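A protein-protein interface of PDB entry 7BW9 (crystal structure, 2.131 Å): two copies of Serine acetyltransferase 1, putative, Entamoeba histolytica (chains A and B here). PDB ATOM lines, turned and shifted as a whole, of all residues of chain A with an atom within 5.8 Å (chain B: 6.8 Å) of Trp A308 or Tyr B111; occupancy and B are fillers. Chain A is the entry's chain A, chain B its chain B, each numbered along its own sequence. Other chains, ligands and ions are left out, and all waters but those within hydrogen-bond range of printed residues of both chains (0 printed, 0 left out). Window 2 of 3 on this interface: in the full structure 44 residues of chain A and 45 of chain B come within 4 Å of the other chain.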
ATOM      1  N   GLU A 304       1.714 -14.828 -23.467  1.00  0.00           N
ATOM      2  CA  GLU A 304       2.904 -13.955 -23.288  1.00  0.00           C
ATOM      3  C   GLU A 304       2.652 -13.018 -22.101  1.00  0.00           C
ATOM      4  O   GLU A 304       3.459 -13.027 -21.178  1.00  0.00           O
ATOM      5  CB  GLU A 304       3.212 -13.198 -24.584  1.00  0.00           C
ATOM      6  CG  GLU A 304       4.612 -12.618 -24.646  1.00  0.00           C
ATOM      7  CD  GLU A 304       5.127 -12.349 -26.049  1.00  0.00           C
ATOM      8  OE1 GLU A 304       4.437 -12.742 -27.010  1.00  0.00           O
ATOM      9  OE2 GLU A 304       6.220 -11.749 -26.183  1.00  0.00           O
ATOM     10  N   ASN A 305       1.544 -12.283 -22.125  1.00  0.00           N
ATOM     11  CA  ASN A 305       1.223 -11.319 -21.043  1.00  0.00           C
ATOM     12  C   ASN A 305       1.146 -12.041 -19.698  1.00  0.00           C
ATOM     13  O   ASN A 305       1.555 -11.456 -18.713  1.00  0.00           O
ATOM     14  CB  ASN A 305      -0.072 -10.555 -21.301  1.00  0.00           C
ATOM     15  CG  ASN A 305      -0.012  -9.714 -22.554  1.00  0.00           C
ATOM     16  OD1 ASN A 305       1.044  -9.579 -23.150  1.00  0.00           O
ATOM     17  ND2 ASN A 305      -1.140  -9.170 -22.967  1.00  0.00           N
ATOM     18  N   LEU A 306       0.623 -13.263 -19.680  1.00  0.00           N
ATOM     19  CA  LEU A 306       0.515 -14.015 -18.406  1.00  0.00           C
ATOM     20  C   LEU A 306       1.912 -14.139 -17.786  1.00  0.00           C
ATOM     21  O   LEU A 306       2.114 -13.638 -16.678  1.00  0.00           O
ATOM     22  CB  LEU A 306      -0.097 -15.381 -18.709  1.00  0.00           C
ATOM     23  CG  LEU A 306      -1.600 -15.493 -18.461  1.00  0.00           C
ATOM     24  CD1 LEU A 306      -2.371 -14.507 -19.314  1.00  0.00           C
ATOM     25  CD2 LEU A 306      -2.082 -16.913 -18.716  1.00  0.00           C
ATOM     26  N   SER A 307       2.843 -14.768 -18.498  1.00  0.00           N
ATOM     27  CA  SER A 307       4.232 -14.915 -17.996  1.00  0.00           C
ATOM     28  C   SER A 307       4.790 -13.532 -17.642  1.00  0.00           C
ATOM     29  O   SER A 307       5.344 -13.372 -16.557  1.00  0.00           O
ATOM     30  CB  SER A 307       5.079 -15.617 -19.011  1.00  0.00           C
ATOM     31  OG  SER A 307       6.424 -15.676 -18.586  1.00  0.00           O
ATOM     32  N   TRP A 308       4.644 -12.571 -18.551  1.00  0.00           N
ATOM     33  CA  TRP A 308       5.118 -11.193 -18.285  1.00  0.00           C
ATOM     34  C   TRP A 308       4.473 -10.636 -17.023  1.00  0.00           C
ATOM     35  O   TRP A 308       5.209 -10.139 -16.235  1.00  0.00           O
ATOM     36  CB  TRP A 308       4.914 -10.261 -19.477  1.00  0.00           C
ATOM     37  CG  TRP A 308       6.223 -10.059 -20.159  1.00  0.00           C
ATOM     38  CD1 TRP A 308       6.532 -10.319 -21.460  1.00  0.00           C
ATOM     39  CD2 TRP A 308       7.438  -9.614 -19.529  1.00  0.00           C
ATOM     40  NE1 TRP A 308       7.856 -10.049 -21.687  1.00  0.00           N
ATOM     41  CE2 TRP A 308       8.436  -9.608 -20.522  1.00  0.00           C
ATOM     42  CE3 TRP A 308       7.777  -9.217 -18.231  1.00  0.00           C
ATOM     43  CZ2 TRP A 308       9.745  -9.217 -20.252  1.00  0.00           C
ATOM     44  CZ3 TRP A 308       9.072  -8.834 -17.966  1.00  0.00           C
ATOM     45  CH2 TRP A 308      10.042  -8.838 -18.965  1.00  0.00           C
ATOM     46  N   VAL A 309       3.167 -10.820 -16.823  1.00  0.00           N
ATOM     47  CA  VAL A 309       2.461 -10.268 -15.628  1.00  0.00           C
ATOM     48  C   VAL A 309       2.891 -10.992 -14.347  1.00  0.00           C
ATOM     49  O   VAL A 309       2.785 -10.383 -13.281  1.00  0.00           O
ATOM     50  CB  VAL A 309       0.932 -10.246 -15.810  1.00  0.00           C
ATOM     51  CG1 VAL A 309       0.209 -10.637 -14.537  1.00  0.00           C
ATOM     52  CG2 VAL A 309       0.444  -8.899 -16.332  1.00  0.00           C
ATOM     53  N   ASN A 310       3.380 -12.230 -14.443  1.00  0.00           N
ATOM     54  CA  ASN A 310       3.893 -12.963 -13.257  1.00  0.00           C
ATOM     55  C   ASN A 310       5.043 -12.161 -12.613  1.00  0.00           C
ATOM     56  O   ASN A 310       5.067 -12.058 -11.396  1.00  0.00           O
ATOM     57  CB  ASN A 310       4.228 -14.423 -13.599  1.00  0.00           C
ATOM     58  CG  ASN A 310       3.020 -15.278 -13.938  1.00  0.00           C
ATOM     59  OD1 ASN A 310       1.889 -14.813 -13.887  1.00  0.00           O
ATOM     60  ND2 ASN A 310       3.235 -16.533 -14.291  1.00  0.00           N
ATOM     61  N   SER A 311       5.926 -11.558 -13.410  1.00  0.00           N
ATOM     62  CA  SER A 311       7.113 -10.791 -12.933  1.00  0.00           C
ATOM     63  C   SER A 311       6.825  -9.570 -12.034  1.00  0.00           C
ATOM     64  O   SER A 311       7.416  -9.517 -10.967  1.00  0.00           O
ATOM     65  CB  SER A 311       7.998 -10.437 -14.085  1.00  0.00           C
ATOM     66  OG  SER A 311       8.295 -11.597 -14.835  1.00  0.00           O
ATOM     67  N   PRO A 312       6.030  -8.542 -12.401  1.00  0.00           N
ATOM     68  CA  PRO A 312       5.818  -7.368 -11.562  1.00  0.00           C
ATOM     69  C   PRO A 312       4.845  -7.714 -10.436  1.00  0.00           C
ATOM     70  O   PRO A 312       4.865  -7.040  -9.442  1.00  0.00           O
ATOM     71  CB  PRO A 312       5.206  -6.326 -12.503  1.00  0.00           C
ATOM     72  CG  PRO A 312       4.420  -7.151 -13.464  1.00  0.00           C
ATOM     73  CD  PRO A 312       5.276  -8.384 -13.620  1.00  0.00           C
ATOM     74  N   ASP B 106       0.055  -2.126 -24.412  1.00  0.00           N
ATOM     75  CA  ASP B 106       1.091  -1.116 -24.617  1.00  0.00           C
ATOM     76  C   ASP B 106       1.948  -0.962 -23.362  1.00  0.00           C
ATOM     77  O   ASP B 106       3.181  -0.943 -23.425  1.00  0.00           O
ATOM     78  CB  ASP B 106       0.441   0.226 -24.998  1.00  0.00           C
ATOM     79  CG  ASP B 106      -0.302   0.181 -26.360  1.00  0.00           C
ATOM     80  OD1 ASP B 106       0.110  -0.577 -27.278  1.00  0.00           O
ATOM     81  OD2 ASP B 106      -1.318   0.907 -26.516  1.00  0.00           O
ATOM     82  N   ILE B 107       1.293  -0.873 -22.203  1.00  0.00           N
ATOM     83  CA  ILE B 107       1.993  -0.745 -20.929  1.00  0.00           C
ATOM     84  C   ILE B 107       2.854  -1.970 -20.664  1.00  0.00           C
ATOM     85  O   ILE B 107       3.978  -1.855 -20.166  1.00  0.00           O
ATOM     86  CB  ILE B 107       0.970  -0.525 -19.795  1.00  0.00           C
ATOM     87  CG1 ILE B 107       0.361   0.871 -19.895  1.00  0.00           C
ATOM     88  CG2 ILE B 107       1.594  -0.773 -18.436  1.00  0.00           C
ATOM     89  CD1 ILE B 107      -1.013   0.984 -19.223  1.00  0.00           C
ATOM     90  N   ILE B 108       2.320  -3.163 -20.951  1.00  0.00           N
ATOM     91  CA  ILE B 108       3.101  -4.392 -20.821  1.00  0.00           C
ATOM     92  C   ILE B 108       4.315  -4.343 -21.747  1.00  0.00           C
ATOM     93  O   ILE B 108       5.420  -4.753 -21.373  1.00  0.00           O
ATOM     94  CB  ILE B 108       2.215  -5.622 -21.118  1.00  0.00           C
ATOM     95  CG1 ILE B 108       1.087  -5.774 -20.086  1.00  0.00           C
ATOM     96  CG2 ILE B 108       3.045  -6.914 -21.212  1.00  0.00           C
ATOM     97  CD1 ILE B 108       1.579  -5.967 -18.693  1.00  0.00           C
ATOM     98  N   ALA B 109       4.127  -3.846 -22.970  1.00  0.00           N
ATOM     99  CA  ALA B 109       5.250  -3.791 -23.905  1.00  0.00           C
ATOM    100  C   ALA B 109       6.323  -2.816 -23.434  1.00  0.00           C
ATOM    101  O   ALA B 109       7.516  -3.069 -23.641  1.00  0.00           O
ATOM    102  CB  ALA B 109       4.761  -3.428 -25.307  1.00  0.00           C
ATOM    103  N   ALA B 110       5.926  -1.722 -22.768  1.00  0.00           N
ATOM    104  CA  ALA B 110       6.904  -0.773 -22.236  1.00  0.00           C
ATOM    105  C   ALA B 110       7.738  -1.407 -21.124  1.00  0.00           C
ATOM    106  O   ALA B 110       8.963  -1.254 -21.087  1.00  0.00           O
ATOM    107  CB  ALA B 110       6.203   0.485 -21.720  1.00  0.00           C
ATOM    108  N   TYR B 111       7.090  -2.114 -20.199  1.00  0.00           N
ATOM    109  CA  TYR B 111       7.833  -2.754 -19.120  1.00  0.00           C
ATOM    110  C   TYR B 111       8.790  -3.809 -19.669  1.00  0.00           C
ATOM    111  O   TYR B 111       9.936  -3.924 -19.213  1.00  0.00           O
ATOM    112  CB  TYR B 111       6.864  -3.370 -18.100  1.00  0.00           C
ATOM    113  CG  TYR B 111       7.597  -4.087 -16.991  1.00  0.00           C
ATOM    114  CD1 TYR B 111       8.203  -3.374 -15.956  1.00  0.00           C
ATOM    115  CD2 TYR B 111       7.720  -5.473 -16.996  1.00  0.00           C
ATOM    116  CE1 TYR B 111       8.897  -4.026 -14.949  1.00  0.00           C
ATOM    117  CE2 TYR B 111       8.412  -6.142 -15.989  1.00  0.00           C
ATOM    118  CZ  TYR B 111       9.001  -5.417 -14.972  1.00  0.00           C
ATOM    119  OH  TYR B 111       9.688  -6.086 -13.974  1.00  0.00           O
ATOM    120  N   THR B 112       8.334  -4.575 -20.658  1.00  0.00           N
ATOM    121  CA  THR B 112       9.160  -5.607 -21.273  1.00  0.00           C
ATOM    122  C   THR B 112      10.327  -5.002 -22.046  1.00  0.00           C
ATOM    123  O   THR B 112      11.453  -5.502 -21.970  1.00  0.00           O
ATOM    124  CB  THR B 112       8.290  -6.463 -22.202  1.00  0.00           C
ATOM    125  OG1 THR B 112       7.319  -7.178 -21.426  1.00  0.00           O
ATOM    126  CG2 THR B 112       9.129  -7.456 -22.982  1.00  0.00           C
ATOM    127  N   GLY B 113      10.078  -3.921 -22.788  1.00  0.00           N
ATOM    128  CA  GLY B 113      11.034  -3.351 -23.708  1.00  0.00           C
ATOM    129  C   GLY B 113      11.997  -2.319 -23.157  1.00  0.00           C
ATOM    130  O   GLY B 113      12.877  -1.871 -23.898  1.00  0.00           O
ATOM    131  N   ASP B 114      11.885  -1.917 -21.896  1.00  0.00           N
ATOM    132  CA  ASP B 114      12.705  -0.826 -21.368  1.00  0.00           C
ATOM    133  C   ASP B 114      13.367  -1.220 -20.053  1.00  0.00           C
ATOM    134  O   ASP B 114      12.672  -1.385 -19.026  1.00  0.00           O
ATOM    135  CB  ASP B 114      11.856   0.429 -21.220  1.00  0.00           C
ATOM    136  CG  ASP B 114      12.620   1.608 -20.645  1.00  0.00           C
ATOM    137  OD1 ASP B 114      13.872   1.550 -20.553  1.00  0.00           O
ATOM    138  OD2 ASP B 114      11.943   2.609 -20.282  1.00  0.00           O
ATOM    139  N   PRO B 115      14.690  -1.372 -20.030  1.00  0.00           N
ATOM    140  CA  PRO B 115      15.366  -1.715 -18.767  1.00  0.00           C
ATOM    141  C   PRO B 115      15.194  -0.660 -17.695  1.00  0.00           C
ATOM    142  O   PRO B 115      15.309  -0.989 -16.515  1.00  0.00           O
ATOM    143  CB  PRO B 115      16.840  -1.864 -19.186  1.00  0.00           C
ATOM    144  CG  PRO B 115      16.774  -2.126 -20.665  1.00  0.00           C
ATOM    145  CD  PRO B 115      15.632  -1.304 -21.158  1.00  0.00           C
ATOM    146  N   ALA B 117      12.400   0.899 -17.040  1.00  0.00           N
ATOM    147  CA  ALA B 117      11.027   0.901 -16.532  1.00  0.00           C
ATOM    148  C   ALA B 117      10.943  -0.020 -15.322  1.00  0.00           C
ATOM    149  O   ALA B 117      11.025  -1.248 -15.458  1.00  0.00           O
ATOM    150  CB  ALA B 117      10.048   0.467 -17.616  1.00  0.00           C
ATOM    151  N   SER B 118      10.746   0.572 -14.144  1.00  0.00           N
ATOM    152  CA  SER B 118      10.829  -0.142 -12.877  1.00  0.00           C
ATOM    153  C   SER B 118       9.491  -0.688 -12.389  1.00  0.00           C
ATOM    154  O   SER B 118       9.472  -1.668 -11.635  1.00  0.00           O
ATOM    155  CB  SER B 118      11.410   0.783 -11.808  1.00  0.00           C
ATOM    156  OG  SER B 118      10.364   1.507 -11.166  1.00  0.00           O
ATOM    157  N   SER B 119       8.375  -0.076 -12.776  1.00  0.00           N
ATOM    158  CA  SER B 119       7.069  -0.496 -12.288  1.00  0.00           C
ATOM    159  C   SER B 119       6.020  -0.012 -13.276  1.00  0.00           C
ATOM    160  O   SER B 119       6.297   0.823 -14.138  1.00  0.00           O
ATOM    161  CB  SER B 119       6.786   0.060 -10.888  1.00  0.00           C
ATOM    162  OG  SER B 119       6.676   1.477 -10.948  1.00  0.00           O
ATOM    163  N   LEU B 120       4.797  -0.533 -13.133  1.00  0.00           N
ATOM    164  CA  LEU B 120       3.734  -0.067 -14.016  1.00  0.00           C
ATOM    165  C   LEU B 120       3.290   1.349 -13.652  1.00  0.00           C
ATOM    166  O   LEU B 120       2.919   2.131 -14.537  1.00  0.00           O
ATOM    167  CB  LEU B 120       2.549  -1.027 -13.972  1.00  0.00           C
ATOM    168  CG  LEU B 120       2.771  -2.461 -14.443  1.00  0.00           C
ATOM    169  CD1 LEU B 120       1.441  -3.068 -14.913  1.00  0.00           C
ATOM    170  CD2 LEU B 120       3.830  -2.545 -15.529  1.00  0.00           C
ATOM    171  N   ILE B 123       5.309   3.746 -15.518  1.00  0.00           N
ATOM    172  CA  ILE B 123       4.968   3.740 -16.935  1.00  0.00           C
ATOM    173  C   ILE B 123       3.635   4.439 -17.164  1.00  0.00           C
ATOM    174  O   ILE B 123       3.508   5.313 -18.030  1.00  0.00           O
ATOM    175  CB  ILE B 123       4.939   2.293 -17.456  1.00  0.00           C
ATOM    176  CG1 ILE B 123       6.326   1.662 -17.326  1.00  0.00           C
ATOM    177  CG2 ILE B 123       4.398   2.249 -18.884  1.00  0.00           C
ATOM    178  CD1 ILE B 123       6.296   0.152 -17.441  1.00  0.00           C
ATOM    179  N   TYR B 127       5.184   7.679 -18.687  1.00  0.00           N
ATOM    180  CA  TYR B 127       5.747   7.343 -20.001  1.00  0.00           C
ATOM    181  C   TYR B 127       4.960   8.052 -21.099  1.00  0.00           C
ATOM    182  O   TYR B 127       3.755   7.799 -21.251  1.00  0.00           O
ATOM    183  CB  TYR B 127       5.769   5.839 -20.235  1.00  0.00           C
ATOM    184  CG  TYR B 127       7.085   5.240 -19.787  1.00  0.00           C
ATOM    185  CD1 TYR B 127       7.627   5.589 -18.553  1.00  0.00           C
ATOM    186  CD2 TYR B 127       7.818   4.374 -20.609  1.00  0.00           C
ATOM    187  CE1 TYR B 127       8.841   5.089 -18.126  1.00  0.00           C
ATOM    188  CE2 TYR B 127       9.037   3.852 -20.184  1.00  0.00           C
ATOM    189  CZ  TYR B 127       9.545   4.224 -18.937  1.00  0.00           C
ATOM    190  OH  TYR B 127      10.743   3.728 -18.468  1.00  0.00           O
ATOM    191  N   PHE B 177       5.224   0.059 -28.394  1.00  0.00           N
ATOM    192  CA  PHE B 177       6.018   0.802 -27.420  1.00  0.00           C
ATOM    193  C   PHE B 177       6.874   1.853 -28.113  1.00  0.00           C
ATOM    194  O   PHE B 177       7.779   1.521 -28.893  1.00  0.00           O
ATOM    195  CB  PHE B 177       6.901  -0.134 -26.592  1.00  0.00           C
ATOM    196  CG  PHE B 177       7.847   0.585 -25.656  1.00  0.00           C
ATOM    197  CD1 PHE B 177       7.442   1.701 -24.958  1.00  0.00           C
ATOM    198  CD2 PHE B 177       9.139   0.124 -25.470  1.00  0.00           C
ATOM    199  CE1 PHE B 177       8.311   2.345 -24.099  1.00  0.00           C
ATOM    200  CE2 PHE B 177      10.017   0.768 -24.611  1.00  0.00           C
ATOM    201  CZ  PHE B 177       9.596   1.873 -23.922  1.00  0.00           C
ATOM    202  N   TRP B 195       3.838  -5.825 -31.327  1.00  0.00           N
ATOM    203  CA  TRP B 195       5.121  -5.910 -30.617  1.00  0.00           C
ATOM    204  C   TRP B 195       6.212  -5.127 -31.338  1.00  0.00           C
ATOM    205  O   TRP B 195       7.357  -5.567 -31.433  1.00  0.00           O
ATOM    206  CB  TRP B 195       5.549  -7.371 -30.392  1.00  0.00           C
ATOM    207  CG  TRP B 195       4.893  -7.967 -29.171  1.00  0.00           C
ATOM    208  CD1 TRP B 195       3.826  -8.819 -29.145  1.00  0.00           C
ATOM    209  CD2 TRP B 195       5.226  -7.700 -27.799  1.00  0.00           C
ATOM    210  NE1 TRP B 195       3.485  -9.111 -27.845  1.00  0.00           N
ATOM    211  CE2 TRP B 195       4.331  -8.447 -26.998  1.00  0.00           C
ATOM    212  CE3 TRP B 195       6.200  -6.913 -27.170  1.00  0.00           C
ATOM    213  CZ2 TRP B 195       4.377  -8.430 -25.601  1.00  0.00           C
ATOM    214  CZ3 TRP B 195       6.248  -6.895 -25.776  1.00  0.00           C
ATOM    215  CH2 TRP B 195       5.339  -7.655 -25.008  1.00  0.00           C
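The side-chain hydroxyl (OG1) of Thr B112 lies close to the indole nitrogen (NE1) of Trp A308 (2.9 Å).
O of Ile B108 sits at hydrogen-bond distance from OG1 of Thr B112, 3.1 Å away.
OE2 of Glu A304 touches CZ2 of Trp B195, at 3.8 Å.
OD1 of Asn A305 touches CG2 of Ile B108, at 3.9 Å.
Trp A308 touches Tyr B111 (CZ3 to CE2, 3.4 Å).
Val A309 touches Ile B108.
Printed residues of chain B within 4 Å of Trp A308: Tyr B111 (3.4 Å) and Thr B112 (2.8 Å).
Of chain A, only Trp A308 comes within 4 Å of Tyr B111.
Printed residues of chain A within 4 Å of Thr B112: Trp A308.
Of the printed residues of chain B, Val A309 touches Ile B108 (3.9 Å).
Of the printed residues of chain B, Glu A304 touches Trp B195.
Printed residues of chain B within 4 Å of Asn A305: Ile B108 (3.9 Å).
Ala B109 touches none of the printed residues of chain A.
Ser A307 touches none of the printed residues of chain B.
The nearest residue of chain B that does not touch Trp A308 is Ile B108 (4.2 Å).
Hydrophobic or aromatic side chains of chain B within 4 Å of the printed part of chain A: Ile B108, Tyr B111 and Trp B195.
Of the 9 printed residues of chain A, 4 touch a printed residue of chain B.
Hydrophobic or aromatic side chains of chain A that line the printed part of chain B: Trp A308 and Val A309.
Along chain A the printed residues that touch a printed residue of chain B span positions 304 to 309.
Among the printed residues, 5 pairs touch across the chains.
No position is printed for both chains.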
